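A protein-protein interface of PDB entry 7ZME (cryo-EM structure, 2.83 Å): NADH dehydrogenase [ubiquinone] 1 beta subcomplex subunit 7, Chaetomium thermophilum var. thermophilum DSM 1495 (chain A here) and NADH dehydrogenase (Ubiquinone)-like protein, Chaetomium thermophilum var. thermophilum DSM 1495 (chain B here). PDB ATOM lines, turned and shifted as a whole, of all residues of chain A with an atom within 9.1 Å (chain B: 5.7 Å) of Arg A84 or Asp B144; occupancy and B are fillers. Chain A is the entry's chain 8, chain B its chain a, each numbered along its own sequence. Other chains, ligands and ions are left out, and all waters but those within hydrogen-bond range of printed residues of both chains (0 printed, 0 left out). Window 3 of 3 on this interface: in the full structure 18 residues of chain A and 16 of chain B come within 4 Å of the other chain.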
ATOM      1  N   VAL A  70       0.298  18.715   7.405  1.00  0.00           N
ATOM      2  CA  VAL A  70       0.234  17.534   8.259  1.00  0.00           C
ATOM      3  C   VAL A  70       0.505  17.895   9.716  1.00  0.00           C
ATOM      4  O   VAL A  70       0.026  17.208  10.624  1.00  0.00           O
ATOM      5  CB  VAL A  70       1.208  16.444   7.776  1.00  0.00           C
ATOM      6  CG1 VAL A  70       0.850  15.988   6.374  1.00  0.00           C
ATOM      7  CG2 VAL A  70       2.644  16.920   7.848  1.00  0.00           C
ATOM      8  N   MET A  73      -2.706  19.169  12.208  1.00  0.00           N
ATOM      9  CA  MET A  73      -3.551  18.309  13.026  1.00  0.00           C
ATOM     10  C   MET A  73      -2.891  17.887  14.329  1.00  0.00           C
ATOM     11  O   MET A  73      -3.564  17.285  15.173  1.00  0.00           O
ATOM     12  CB  MET A  73      -3.966  17.055  12.257  1.00  0.00           C
ATOM     13  CG  MET A  73      -5.057  17.292  11.244  1.00  0.00           C
ATOM     14  SD  MET A  73      -4.367  18.176   9.850  1.00  0.00           S
ATOM     15  CE  MET A  73      -3.456  16.826   9.131  1.00  0.00           C
ATOM     16  N   LEU A  76      -5.062  19.651  16.063  1.00  0.00           N
ATOM     17  CA  LEU A  76      -6.437  19.275  15.748  1.00  0.00           C
ATOM     18  C   LEU A  76      -6.764  17.861  16.216  1.00  0.00           C
ATOM     19  O   LEU A  76      -7.854  17.619  16.746  1.00  0.00           O
ATOM     20  CB  LEU A  76      -6.689  19.409  14.246  1.00  0.00           C
ATOM     21  CG  LEU A  76      -8.109  19.101  13.769  1.00  0.00           C
ATOM     22  CD1 LEU A  76      -9.102  20.069  14.390  1.00  0.00           C
ATOM     23  CD2 LEU A  76      -8.188  19.147  12.252  1.00  0.00           C
ATOM     24  N   ARG A  77      -5.842  16.913  16.021  1.00  0.00           N
ATOM     25  CA  ARG A  77      -6.095  15.542  16.456  1.00  0.00           C
ATOM     26  C   ARG A  77      -6.235  15.459  17.970  1.00  0.00           C
ATOM     27  O   ARG A  77      -7.124  14.768  18.482  1.00  0.00           O
ATOM     28  CB  ARG A  77      -4.980  14.616  15.970  1.00  0.00           C
ATOM     29  CG  ARG A  77      -4.944  14.426  14.463  1.00  0.00           C
ATOM     30  CD  ARG A  77      -3.655  13.753  14.019  1.00  0.00           C
ATOM     31  NE  ARG A  77      -3.650  12.322  14.310  1.00  0.00           N
ATOM     32  CZ  ARG A  77      -4.182  11.399  13.517  1.00  0.00           C
ATOM     33  NH1 ARG A  77      -4.133  10.119  13.859  1.00  0.00           N
ATOM     34  NH2 ARG A  77      -4.765  11.755  12.379  1.00  0.00           N
ATOM     35  N   LYS A  80      -9.597  16.635  19.203  1.00  0.00           N
ATOM     36  CA  LYS A  80     -10.608  15.590  19.148  1.00  0.00           C
ATOM     37  C   LYS A  80     -10.213  14.353  19.941  1.00  0.00           C
ATOM     38  O   LYS A  80     -10.943  13.357  19.913  1.00  0.00           O
ATOM     39  CB  LYS A  80     -10.889  15.201  17.694  1.00  0.00           C
ATOM     40  CG  LYS A  80     -11.534  16.301  16.869  1.00  0.00           C
ATOM     41  CD  LYS A  80     -11.891  15.806  15.478  1.00  0.00           C
ATOM     42  CE  LYS A  80     -12.445  16.930  14.618  1.00  0.00           C
ATOM     43  NZ  LYS A  80     -13.746  17.433  15.135  1.00  0.00           N
ATOM     44  N   GLY A  81      -9.083  14.391  20.641  1.00  0.00           N
ATOM     45  CA  GLY A  81      -8.627  13.243  21.405  1.00  0.00           C
ATOM     46  C   GLY A  81      -8.253  12.045  20.560  1.00  0.00           C
ATOM     47  O   GLY A  81      -8.573  10.908  20.929  1.00  0.00           O
ATOM     48  N   GLY A  82      -7.580  12.271  19.435  1.00  0.00           N
ATOM     49  CA  GLY A  82      -7.201  11.174  18.559  1.00  0.00           C
ATOM     50  C   GLY A  82      -8.381  10.437  17.962  1.00  0.00           C
ATOM     51  O   GLY A  82      -8.359   9.204  17.871  1.00  0.00           O
ATOM     52  N   ALA A  83      -9.413  11.168  17.551  1.00  0.00           N
ATOM     53  CA  ALA A  83     -10.596  10.565  16.963  1.00  0.00           C
ATOM     54  C   ALA A  83     -10.423  10.433  15.451  1.00  0.00           C
ATOM     55  O   ALA A  83      -9.367  10.729  14.889  1.00  0.00           O
ATOM     56  CB  ALA A  83     -11.839  11.382  17.309  1.00  0.00           C
ATOM     57  N   ARG A  84     -11.481   9.982  14.781  1.00  0.00           N
ATOM     58  CA  ARG A  84     -11.473   9.812  13.331  1.00  0.00           C
ATOM     59  C   ARG A  84     -11.810  11.154  12.693  1.00  0.00           C
ATOM     60  O   ARG A  84     -12.976  11.555  12.643  1.00  0.00           O
ATOM     61  CB  ARG A  84     -12.457   8.729  12.906  1.00  0.00           C
ATOM     62  CG  ARG A  84     -12.416   7.477  13.764  1.00  0.00           C
ATOM     63  CD  ARG A  84     -11.149   6.686  13.509  1.00  0.00           C
ATOM     64  NE  ARG A  84     -10.948   6.426  12.087  1.00  0.00           N
ATOM     65  CZ  ARG A  84      -9.839   5.904  11.576  1.00  0.00           C
ATOM     66  NH1 ARG A  84      -8.829   5.582  12.373  1.00  0.00           N
ATOM     67  NH2 ARG A  84      -9.737   5.703  10.270  1.00  0.00           N
ATOM     68  N   SER A  85     -10.788  11.852  12.202  1.00  0.00           N
ATOM     69  CA  SER A  85     -10.997  13.146  11.565  1.00  0.00           C
ATOM     70  C   SER A  85     -11.506  13.028  10.135  1.00  0.00           C
ATOM     71  O   SER A  85     -11.945  14.034   9.568  1.00  0.00           O
ATOM     72  CB  SER A  85      -9.700  13.957  11.584  1.00  0.00           C
ATOM     73  OG  SER A  85      -8.695  13.332  10.806  1.00  0.00           O
ATOM     74  N   ASN A  86     -11.459  11.840   9.542  1.00  0.00           N
ATOM     75  CA  ASN A  86     -11.932  11.646   8.176  1.00  0.00           C
ATOM     76  C   ASN A  86     -13.379  11.165   8.161  1.00  0.00           C
ATOM     77  O   ASN A  86     -13.837  10.517   9.102  1.00  0.00           O
ATOM     78  CB  ASN A  86     -11.038  10.654   7.432  1.00  0.00           C
ATOM     79  CG  ASN A  86     -11.080   9.264   8.036  1.00  0.00           C
ATOM     80  OD1 ASN A  86     -11.361   9.097   9.223  1.00  0.00           O
ATOM     81  ND2 ASN A  86     -10.800   8.256   7.219  1.00  0.00           N
ATOM     82  N   TYR B 142      -8.470   1.284  10.025  1.00  0.00           N
ATOM     83  CA  TYR B 142      -7.989   1.967   8.837  1.00  0.00           C
ATOM     84  C   TYR B 142      -7.459   3.339   9.230  1.00  0.00           C
ATOM     85  O   TYR B 142      -8.063   4.023  10.064  1.00  0.00           O
ATOM     86  CB  TYR B 142      -9.087   2.096   7.767  1.00  0.00           C
ATOM     87  CG  TYR B 142     -10.210   3.058   8.083  1.00  0.00           C
ATOM     88  CD1 TYR B 142     -11.052   2.847   9.167  1.00  0.00           C
ATOM     89  CD2 TYR B 142     -10.448   4.163   7.275  1.00  0.00           C
ATOM     90  CE1 TYR B 142     -12.087   3.718   9.449  1.00  0.00           C
ATOM     91  CE2 TYR B 142     -11.478   5.039   7.549  1.00  0.00           C
ATOM     92  CZ  TYR B 142     -12.293   4.813   8.635  1.00  0.00           C
ATOM     93  OH  TYR B 142     -13.322   5.685   8.911  1.00  0.00           O
ATOM     94  N   PRO B 143      -6.336   3.760   8.657  1.00  0.00           N
ATOM     95  CA  PRO B 143      -5.645   4.947   9.170  1.00  0.00           C
ATOM     96  C   PRO B 143      -6.435   6.226   8.956  1.00  0.00           C
ATOM     97  O   PRO B 143      -7.203   6.364   8.000  1.00  0.00           O
ATOM     98  CB  PRO B 143      -4.339   4.965   8.369  1.00  0.00           C
ATOM     99  CG  PRO B 143      -4.683   4.271   7.100  1.00  0.00           C
ATOM    100  CD  PRO B 143      -5.665   3.199   7.473  1.00  0.00           C
ATOM    101  N   ASP B 144      -6.235   7.168   9.873  1.00  0.00           N
ATOM    102  CA  ASP B 144      -6.780   8.505   9.719  1.00  0.00           C
ATOM    103  C   ASP B 144      -5.997   9.271   8.654  1.00  0.00           C
ATOM    104  O   ASP B 144      -4.871   8.915   8.299  1.00  0.00           O
ATOM    105  CB  ASP B 144      -6.734   9.254  11.052  1.00  0.00           C
ATOM    106  CG  ASP B 144      -7.626  10.478  11.066  1.00  0.00           C
ATOM    107  OD1 ASP B 144      -8.855  10.320  11.221  1.00  0.00           O
ATOM    108  OD2 ASP B 144      -7.097  11.602  10.923  1.00  0.00           O
ATOM    109  N   ARG B 145      -6.613  10.331   8.138  1.00  0.00           N
ATOM    110  CA  ARG B 145      -5.974  11.119   7.094  1.00  0.00           C
ATOM    111  C   ARG B 145      -4.729  11.810   7.634  1.00  0.00           C
ATOM    112  O   ARG B 145      -4.635  12.141   8.819  1.00  0.00           O
ATOM    113  CB  ARG B 145      -6.949  12.147   6.523  1.00  0.00           C
ATOM    114  CG  ARG B 145      -7.412  13.205   7.503  1.00  0.00           C
ATOM    115  CD  ARG B 145      -8.404  14.137   6.832  1.00  0.00           C
ATOM    116  NE  ARG B 145      -7.800  14.844   5.706  1.00  0.00           N
ATOM    117  CZ  ARG B 145      -8.489  15.387   4.709  1.00  0.00           C
ATOM    118  NH1 ARG B 145      -7.855  16.010   3.724  1.00  0.00           N
ATOM    119  NH2 ARG B 145      -9.812  15.306   4.694  1.00  0.00           N
ATOM    120  N   VAL B 146      -3.762  12.024   6.747  1.00  0.00           N
ATOM    121  CA  VAL B 146      -2.443  12.498   7.136  1.00  0.00           C
ATOM    122  C   VAL B 146      -2.316  14.010   6.995  1.00  0.00           C
ATOM    123  O   VAL B 146      -1.655  14.654   7.810  1.00  0.00           O
ATOM    124  CB  VAL B 146      -1.359  11.765   6.315  1.00  0.00           C
ATOM    125  CG1 VAL B 146       0.004  12.403   6.523  1.00  0.00           C
ATOM    126  CG2 VAL B 146      -1.318  10.299   6.701  1.00  0.00           C
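O of Tyr B142 is in hydrogen-bond range of NH1 of Arg A84.
NH2 of Arg A84 lies within hydrogen-bond range of O of Pro B143, 3.5 Å away.
The side-chain carboxylate (OD2) of Asp B144 is in salt-bridge range of the guanidinium group (NH2) of Arg A77, 2.8 Å away.
The side-chain carboxylate of Asp B144 sits at hydrogen-bond distance from the backbone NH of Ser A85 (2.7 Å).
OD1 of Asn A86 sits close to OD1 of Asp B144 (3.4 Å).
The backbone carbonyl oxygen of Arg A77 is in hydrogen-bond range of the backbone NH of Gly A82 (2.7 Å).
Among the printed residues, merely in contact across the chains: Met A73 with Val B146 (3.1 Å), Val A70 with Val B146 (3.2 Å), Asn A86 with Tyr B142 (3.3 Å), Arg A84 with Asp B144 (3.4 Å), Ser A85 with Arg B145 (3.5 Å), Arg A77 with Arg B145 (3.6 Å) and Ala A83 with Asp B144 (3.7 Å).
Arg A84 touches just these residues of chain B: Tyr B142, Pro B143 and Asp B144.
Asp B144 touches just these residues of chain A: Arg A77 (2.8 Å), Ala A83 (3.7 Å), Arg A84 (3.4 Å), Ser A85 (2.4 Å) and Asn A86 (3.4 Å).
Tyr B142 touches just these residues of chain A: Arg A84 (2.4 Å) and Asn A86 (3.3 Å).
Printed residues of chain A within 4 Å of Pro B143: Arg A84.
Of the printed residues of chain B, Val A70 touches Val B146.
Printed residues of chain B within 4 Å of Arg A77: Asp B144 and Arg B145.
Gly A82 touches none of the printed residues of chain B.
Lys A80 touches none of the printed residues of chain B.
The nearest printed residue of chain B that does not touch Arg A84 is Arg B145 (6.0 Å).
The nearest residue of chain A that does not touch Asp B144 is Met A73 (6.1 Å).
Of the 11 printed residues of chain A, 7 touch a printed residue of chain B.
Printed residues of chain A that touch a printed residue of chain B: Val A70, Met A73, Arg A77, Ala A83, Arg A84, Ser A85 and Asn A86.
Hydrophobic or aromatic side chains of chain A within 4 Å of the printed part of chain B: Val A70 and Met A73.
Of the 5 printed residues of chain B, 5 touch a printed residue of chain A.
Printed residues of chain B that touch a printed residue of chain A: Tyr B142, Pro B143, Asp B144, Arg B145 and Val B146.
Hydrophobic or aromatic side chains of chain B within 4 Å of the printed part of chain A: Tyr B142 and Val B146.
Among the printed residues, Asp or Glu carboxylates within 4 Å of a Lys or Arg side-chain nitrogen of the other chain: Arg A77 with Asp B144 (2.8 Å).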
